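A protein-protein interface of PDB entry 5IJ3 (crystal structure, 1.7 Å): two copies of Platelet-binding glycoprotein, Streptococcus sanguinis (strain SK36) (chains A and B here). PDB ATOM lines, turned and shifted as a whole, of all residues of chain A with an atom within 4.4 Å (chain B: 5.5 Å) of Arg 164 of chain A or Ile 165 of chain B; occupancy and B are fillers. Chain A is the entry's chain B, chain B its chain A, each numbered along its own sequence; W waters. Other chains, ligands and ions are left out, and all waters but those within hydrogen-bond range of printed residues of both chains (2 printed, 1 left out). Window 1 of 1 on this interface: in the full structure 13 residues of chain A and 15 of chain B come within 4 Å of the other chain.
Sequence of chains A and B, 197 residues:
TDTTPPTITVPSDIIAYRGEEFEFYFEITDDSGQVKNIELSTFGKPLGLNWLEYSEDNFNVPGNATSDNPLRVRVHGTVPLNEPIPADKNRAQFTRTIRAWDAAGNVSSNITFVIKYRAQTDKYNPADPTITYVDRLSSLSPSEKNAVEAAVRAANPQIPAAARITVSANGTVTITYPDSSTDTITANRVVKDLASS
Water W2 bridges the backbone NH (N) of Ile 165 of chain A (2.9 Å) and the side-chain amide oxygen (OD1) of Asn 146 of chain B (3.3 Å).
Water W1 lies within hydrogen-bond range of NH2 of Arg 164 of chain B and NH2 of Arg 164 of chain A.
Arg 164 of chain A touches Ile 165 of chain B, and with the chains exchanged Ile 165 of chain A touches Arg 164 of chain B.
Arg 164 of chain A touches just these residues of chain B: Pro 142 (3.98 Å), Lys 145 (3.4 Å), Asn 146 (2.9 Å), Glu 149 (2.9 Å), Ile 165 (3.9 Å) and Val 167 (3.9 Å).
Printed residues of chain B within 4 Å of Ala 163 of chain A: Asn 146 (2.9 Å).
Of the printed residues of chain A, Asn 146 of chain B touches Ala 162, Ala 163 and Arg 164.
Of the printed residues of chain B, Ile 165 of chain A touches Arg 164.
Printed residues of chain B within 4 Å of Thr 176 of chain A: Pro 142 (3.7 Å).
Printed residues of chain A within 4 Å of Arg 164 of chain B: Ile 165 (3.9 Å).
Ala 163 of chain B touches none of the printed residues of chain A.
NH1 of Arg 164 of chain A is in hydrogen-bond range of O of Lys 145 of chain B.
The backbone carbonyl oxygen of Ala 162 of chain A lies within hydrogen-bond range of the side-chain amide nitrogen of Asn 146 of chain B, 3.5 Å away.
The side-chain amide nitrogen of Asn 146 of chain B is in hydrogen-bond range of the backbone carbonyl oxygen of Ala 163 of chain A (2.9 Å).
The side-chain amide oxygen (OD1) of Asn 146 of chain B lies within hydrogen-bond range of the guanidinium group (NH1) of Arg 164 of chain A (2.9 Å).
The guanidinium group of Arg 164 of chain A lies close to the side-chain carboxylate of Glu 149 of chain B.
Of the 15 printed residues of chain B, 7 touch a printed residue of chain A.
Of the 8 printed residues of chain A, 5 touch a printed residue of chain B.
Among the printed residues, 11 pairs touch across the chains.
Among the printed residues, Asp or Glu carboxylates within 4 Å of a Lys or Arg side-chain nitrogen of the other chain: Arg 164 of chain A with Glu 149 of chain B (2.9 Å).
O of Ala 162 of chain A touches CB of Pro 142 of chain B, 3.5 Å away.
CD of Arg 164 of chain A touches O of Pro 142 of chain B, 3.98 Å away.
Ile 165 of chain B touches Arg 164 of chain A (O to NH2, 3.9 Å).
NH2 of Arg 164 of chain A touches CG2 of Val 167 of chain B (3.9 Å).
O of Ile 165 of chain A touches NH2 of Arg 164 of chain B, at 3.9 Å.
Pro 142 of chain B touches Thr 176 of chain A (CB to O, 3.7 Å).
The backbone NH (N) of Arg 164 of chain B lies within hydrogen-bond range of the backbone carbonyl oxygen (O) of Thr 176 of chain B, at 2.8 Å.
The backbone carbonyl oxygen of Arg 164 of chain A sits at hydrogen-bond distance from the backbone NH of Thr 176 of chain A.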
ATOM      1  N   ALA A 162     -16.814  15.924  26.552  1.00  0.00           N
ATOM      2  CA  ALA A 162     -17.908  15.740  27.499  1.00  0.00           C
ATOM      3  C   ALA A 162     -18.793  16.979  27.648  1.00  0.00           C
ATOM      4  O   ALA A 162     -19.881  16.898  28.213  1.00  0.00           O
ATOM      5  CB  ALA A 162     -17.350  15.335  28.858  1.00  0.00           C
ATOM      6  N   ALA A 163     -18.329  18.126  27.163  1.00  0.00           N
ATOM      7  CA  ALA A 163     -19.161  19.320  27.160  1.00  0.00           C
ATOM      8  C   ALA A 163     -20.314  19.095  26.201  1.00  0.00           C
ATOM      9  O   ALA A 163     -20.146  18.430  25.179  1.00  0.00           O
ATOM     10  CB  ALA A 163     -18.360  20.549  26.755  1.00  0.00           C
ATOM     11  N   ARG A 164     -21.477  19.643  26.531  1.00  0.00           N
ATOM     12  CA  ARG A 164     -22.632  19.505  25.654  1.00  0.00           C
ATOM     13  C   ARG A 164     -23.003  20.827  25.006  1.00  0.00           C
ATOM     14  O   ARG A 164     -23.181  21.846  25.675  1.00  0.00           O
ATOM     15  CB  ARG A 164     -23.835  18.948  26.408  1.00  0.00           C
ATOM     16  CG  ARG A 164     -25.017  18.647  25.486  1.00  0.00           C
ATOM     17  CD  ARG A 164     -25.904  17.604  26.096  1.00  0.00           C
ATOM     18  NE  ARG A 164     -27.073  17.302  25.269  1.00  0.00           N
ATOM     19  CZ  ARG A 164     -27.082  16.422  24.273  1.00  0.00           C
ATOM     20  NH1 ARG A 164     -25.979  15.758  23.957  1.00  0.00           N
ATOM     21  NH2 ARG A 164     -28.203  16.211  23.591  1.00  0.00           N
ATOM     22  N   ILE A 165     -23.143  20.780  23.688  1.00  0.00           N
ATOM     23  CA  ILE A 165     -23.458  21.950  22.893  1.00  0.00           C
ATOM     24  C   ILE A 165     -24.932  21.926  22.498  1.00  0.00           C
ATOM     25  O   ILE A 165     -25.366  21.011  21.810  1.00  0.00           O
ATOM     26  CB  ILE A 165     -22.591  21.999  21.630  1.00  0.00           C
ATOM     27  CG1 ILE A 165     -21.103  21.974  22.002  1.00  0.00           C
ATOM     28  CG2 ILE A 165     -22.930  23.222  20.804  1.00  0.00           C
ATOM     29  CD1 ILE A 165     -20.189  21.694  20.826  1.00  0.00           C
ATOM     30  N   THR A 166     -25.693  22.924  22.939  1.00  0.00           N
ATOM     31  CA  THR A 166     -27.099  23.027  22.561  1.00  0.00           C
ATOM     32  C   THR A 166     -27.329  24.261  21.689  1.00  0.00           C
ATOM     33  O   THR A 166     -26.581  25.238  21.755  1.00  0.00           O
ATOM     34  CB  THR A 166     -28.020  23.078  23.795  1.00  0.00           C
ATOM     35  OG1 THR A 166     -27.511  24.033  24.737  1.00  0.00           O
ATOM     36  CG2 THR A 166     -28.085  21.711  24.463  1.00  0.00           C
ATOM     37  N   THR A 174     -25.367  27.358  23.349  1.00  0.00           N
ATOM     38  CA  THR A 174     -24.955  27.202  24.738  1.00  0.00           C
ATOM     39  C   THR A 174     -23.994  26.027  24.839  1.00  0.00           C
ATOM     40  O   THR A 174     -24.280  24.945  24.333  1.00  0.00           O
ATOM     41  CB  THR A 174     -26.158  26.972  25.677  1.00  0.00           C
ATOM     42  OG1 THR A 174     -27.049  28.089  25.591  1.00  0.00           O
ATOM     43  CG2 THR A 174     -25.703  26.814  27.118  1.00  0.00           C
ATOM     44  N   ILE A 175     -22.849  26.247  25.474  1.00  0.00           N
ATOM     45  CA  ILE A 175     -21.912  25.174  25.745  1.00  0.00           C
ATOM     46  C   ILE A 175     -21.914  24.943  27.244  1.00  0.00           C
ATOM     47  O   ILE A 175     -21.593  25.847  28.006  1.00  0.00           O
ATOM     48  CB  ILE A 175     -20.488  25.507  25.252  1.00  0.00           C
ATOM     49  CG1 ILE A 175     -20.497  25.765  23.741  1.00  0.00           C
ATOM     50  CG2 ILE A 175     -19.526  24.389  25.595  1.00  0.00           C
ATOM     51  CD1 ILE A 175     -19.143  26.147  23.181  1.00  0.00           C
ATOM     52  N   THR A 176     -22.320  23.746  27.660  1.00  0.00           N
ATOM     53  CA  THR A 176     -22.364  23.397  29.073  1.00  0.00           C
ATOM     54  C   THR A 176     -21.214  22.449  29.396  1.00  0.00           C
ATOM     55  O   THR A 176     -21.180  21.312  28.935  1.00  0.00           O
ATOM     56  CB  THR A 176     -23.714  22.749  29.461  1.00  0.00           C
ATOM     57  OG1 THR A 176     -24.787  23.632  29.105  1.00  0.00           O
ATOM     58  CG2 THR A 176     -23.770  22.464  30.964  1.00  0.00           C
ATOM     59  N   PRO B 142     -23.747  16.694  31.552  1.00  0.00           N
ATOM     60  CA  PRO B 142     -23.549  16.927  30.117  1.00  0.00           C
ATOM     61  C   PRO B 142     -22.976  15.710  29.388  1.00  0.00           C
ATOM     62  O   PRO B 142     -23.422  15.401  28.286  1.00  0.00           O
ATOM     63  CB  PRO B 142     -22.568  18.102  30.086  1.00  0.00           C
ATOM     64  CG  PRO B 142     -22.850  18.842  31.350  1.00  0.00           C
ATOM     65  CD  PRO B 142     -23.182  17.785  32.370  1.00  0.00           C
ATOM     66  N   LYS B 145     -25.703  13.118  28.867  1.00  0.00           N
ATOM     67  CA  LYS B 145     -26.612  13.455  27.773  1.00  0.00           C
ATOM     68  C   LYS B 145     -25.947  13.202  26.421  1.00  0.00           C
ATOM     69  O   LYS B 145     -26.590  12.691  25.502  1.00  0.00           O
ATOM     70  CB  LYS B 145     -27.083  14.904  27.873  1.00  0.00           C
ATOM     71  CG  LYS B 145     -27.963  15.181  29.070  1.00  0.00           C
ATOM     72  CD  LYS B 145     -28.411  16.623  29.112  1.00  0.00           C
ATOM     73  CE  LYS B 145     -29.097  16.921  30.440  1.00  0.00           C
ATOM     74  NZ  LYS B 145     -29.456  18.361  30.592  1.00  0.00           N
ATOM     75  N   ASN B 146     -24.670  13.559  26.298  1.00  0.00           N
ATOM     76  CA  ASN B 146     -23.905  13.219  25.099  1.00  0.00           C
ATOM     77  C   ASN B 146     -23.926  11.718  24.836  1.00  0.00           C
ATOM     78  O   ASN B 146     -24.113  11.275  23.699  1.00  0.00           O
ATOM     79  CB  ASN B 146     -22.444  13.677  25.224  1.00  0.00           C
ATOM     80  CG  ASN B 146     -22.256  15.167  24.984  1.00  0.00           C
ATOM     81  OD1 ASN B 146     -23.192  15.890  24.640  1.00  0.00           O
ATOM     82  ND2 ASN B 146     -21.021  15.637  25.175  1.00  0.00           N
ATOM     83  N   GLU B 149     -27.430  10.547  23.674  1.00  0.00           N
ATOM     84  CA  GLU B 149     -27.623  10.926  22.271  1.00  0.00           C
ATOM     85  C   GLU B 149     -26.836   9.984  21.354  1.00  0.00           C
ATOM     86  O   GLU B 149     -27.356   9.504  20.345  1.00  0.00           O
ATOM     87  CB  GLU B 149     -27.210  12.390  22.022  1.00  0.00           C
ATOM     88  CG  GLU B 149     -27.402  12.876  20.565  1.00  0.00           C
ATOM     89  CD  GLU B 149     -26.943  14.328  20.312  1.00  0.00           C
ATOM     90  OE1 GLU B 149     -26.738  15.103  21.266  1.00  0.00           O
ATOM     91  OE2 GLU B 149     -26.790  14.715  19.135  1.00  0.00           O
ATOM     92  N   VAL B 152     -28.552   6.530  21.260  1.00  0.00           N
ATOM     93  CA  VAL B 152     -29.751   6.554  20.431  1.00  0.00           C
ATOM     94  C   VAL B 152     -29.368   6.585  18.954  1.00  0.00           C
ATOM     95  O   VAL B 152     -29.951   5.873  18.134  1.00  0.00           O
ATOM     96  CB  VAL B 152     -30.649   7.764  20.756  1.00  0.00           C
ATOM     97  CG1 VAL B 152     -31.825   7.839  19.779  1.00  0.00           C
ATOM     98  CG2 VAL B 152     -31.143   7.692  22.188  1.00  0.00           C
ATOM     99  N   ARG B 153     -28.376   7.408  18.628  1.00  0.00           N
ATOM    100  CA  ARG B 153     -27.871   7.526  17.264  1.00  0.00           C
ATOM    101  C   ARG B 153     -27.302   6.193  16.781  1.00  0.00           C
ATOM    102  O   ARG B 153     -27.543   5.773  15.648  1.00  0.00           O
ATOM    103  CB  ARG B 153     -26.804   8.625  17.185  1.00  0.00           C
ATOM    104  CG  ARG B 153     -26.236   8.877  15.796  1.00  0.00           C
ATOM    105  CD  ARG B 153     -27.276   9.454  14.845  1.00  0.00           C
ATOM    106  NE  ARG B 153     -27.658  10.822  15.189  1.00  0.00           N
ATOM    107  CZ  ARG B 153     -28.545  11.539  14.506  1.00  0.00           C
ATOM    108  NH1 ARG B 153     -29.142  11.017  13.439  1.00  0.00           N
ATOM    109  NH2 ARG B 153     -28.839  12.775  14.884  1.00  0.00           N
ATOM    110  N   ALA B 163     -31.939  14.483  11.289  1.00  0.00           N
ATOM    111  CA  ALA B 163     -32.810  14.450  12.457  1.00  0.00           C
ATOM    112  C   ALA B 163     -31.996  14.861  13.675  1.00  0.00           C
ATOM    113  O   ALA B 163     -30.819  14.509  13.792  1.00  0.00           O
ATOM    114  CB  ALA B 163     -33.408  13.073  12.654  1.00  0.00           C
ATOM    115  N   ARG B 164     -32.615  15.611  14.578  1.00  0.00           N
ATOM    116  CA  ARG B 164     -31.899  16.069  15.766  1.00  0.00           C
ATOM    117  C   ARG B 164     -32.365  15.326  17.010  1.00  0.00           C
ATOM    118  O   ARG B 164     -33.562  15.243  17.284  1.00  0.00           O
ATOM    119  CB  ARG B 164     -32.072  17.576  15.950  1.00  0.00           C
ATOM    120  CG  ARG B 164     -31.275  18.138  17.124  1.00  0.00           C
ATOM    121  CD  ARG B 164     -30.926  19.594  16.900  1.00  0.00           C
ATOM    122  NE  ARG B 164     -30.146  20.145  18.009  1.00  0.00           N
ATOM    123  CZ  ARG B 164     -28.827  20.027  18.121  1.00  0.00           C
ATOM    124  NH1 ARG B 164     -28.136  19.374  17.196  1.00  0.00           N
ATOM    125  NH2 ARG B 164     -28.199  20.561  19.168  1.00  0.00           N
ATOM    126  N   ILE B 165     -31.407  14.775  17.751  1.00  0.00           N
ATOM    127  CA  ILE B 165     -31.694  14.048  18.979  1.00  0.00           C
ATOM    128  C   ILE B 165     -31.403  14.925  20.192  1.00  0.00           C
ATOM    129  O   ILE B 165     -30.276  15.386  20.370  1.00  0.00           O
ATOM    130  CB  ILE B 165     -30.858  12.756  19.081  1.00  0.00           C
ATOM    131  CG1 ILE B 165     -31.080  11.873  17.852  1.00  0.00           C
ATOM    132  CG2 ILE B 165     -31.201  11.996  20.352  1.00  0.00           C
ATOM    133  CD1 ILE B 165     -30.061  10.769  17.704  1.00  0.00           C
ATOM    134  N   THR B 166     -32.419  15.159  21.016  1.00  0.00           N
ATOM    135  CA  THR B 166     -32.241  15.930  22.241  1.00  0.00           C
ATOM    136  C   THR B 166     -32.550  15.068  23.456  1.00  0.00           C
ATOM    137  O   THR B 166     -33.281  14.078  23.359  1.00  0.00           O
ATOM    138  CB  THR B 166     -33.128  17.200  22.269  1.00  0.00           C
ATOM    139  OG1 THR B 166     -34.477  16.859  21.917  1.00  0.00           O
ATOM    140  CG2 THR B 166     -32.606  18.237  21.289  1.00  0.00           C
ATOM    141  N   VAL B 167     -31.972  15.451  24.595  1.00  0.00           N
ATOM    142  CA  VAL B 167     -32.095  14.705  25.842  1.00  0.00           C
ATOM    143  C   VAL B 167     -32.442  15.632  27.001  1.00  0.00           C
ATOM    144  O   VAL B 167     -31.775  16.646  27.210  1.00  0.00           O
ATOM    145  CB  VAL B 167     -30.783  13.962  26.189  1.00  0.00           C
ATOM    146  CG1 VAL B 167     -30.992  13.039  27.389  1.00  0.00           C
ATOM    147  CG2 VAL B 167     -30.277  13.186  24.992  1.00  0.00           C
ATOM    148  N   VAL B 173     -35.699  11.096  25.807  1.00  0.00           N
ATOM    149  CA  VAL B 173     -35.145  11.344  24.480  1.00  0.00           C
ATOM    150  C   VAL B 173     -36.206  11.859  23.522  1.00  0.00           C
ATOM    151  O   VAL B 173     -37.299  11.305  23.448  1.00  0.00           O
ATOM    152  CB  VAL B 173     -34.512  10.069  23.886  1.00  0.00           C
ATOM    153  CG1 VAL B 173     -34.147  10.269  22.422  1.00  0.00           C
ATOM    154  CG2 VAL B 173     -33.282   9.670  24.685  1.00  0.00           C
ATOM    155  N   THR B 174     -35.883  12.930  22.805  1.00  0.00           N
ATOM    156  CA  THR B 174     -36.732  13.400  21.718  1.00  0.00           C
ATOM    157  C   THR B 174     -35.965  13.309  20.409  1.00  0.00           C
ATOM    158  O   THR B 174     -34.851  13.819  20.301  1.00  0.00           O
ATOM    159  CB  THR B 174     -37.203  14.849  21.936  1.00  0.00           C
ATOM    160  OG1 THR B 174     -37.950  14.939  23.154  1.00  0.00           O
ATOM    161  CG2 THR B 174     -38.079  15.306  20.773  1.00  0.00           C
ATOM    162  N   ILE B 175     -36.547  12.639  19.423  1.00  0.00           N
ATOM    163  CA  ILE B 175     -35.981  12.631  18.085  1.00  0.00           C
ATOM    164  C   ILE B 175     -36.833  13.525  17.201  1.00  0.00           C
ATOM    165  O   ILE B 175     -38.003  13.234  16.971  1.00  0.00           O
ATOM    166  CB  ILE B 175     -35.921  11.216  17.488  1.00  0.00           C
ATOM    167  CG1 ILE B 175     -35.036  10.310  18.352  1.00  0.00           C
ATOM    168  CG2 ILE B 175     -35.404  11.269  16.060  1.00  0.00           C
ATOM    169  CD1 ILE B 175     -35.115   8.845  17.982  1.00  0.00           C
ATOM    170  N   THR B 176     -36.262  14.626  16.731  1.00  0.00           N
ATOM    171  CA  THR B 176     -37.007  15.540  15.878  1.00  0.00           C
ATOM    172  C   THR B 176     -36.523  15.402  14.444  1.00  0.00           C
ATOM    173  O   THR B 176     -35.393  15.755  14.123  1.00  0.00           O
ATOM    174  CB  THR B 176     -36.874  16.998  16.338  1.00  0.00           C
ATOM    175  OG1 THR B 176     -37.285  17.107  17.708  1.00  0.00           O
ATOM    176  CG2 THR B 176     -37.749  17.902  15.485  1.00  0.00           C
HETATM  177  O   HOH W   1     -28.950  19.018  21.965  1.00  0.00           O
HETATM  178  O   HOH W   2     -22.761  18.223  22.375  1.00  0.00           O
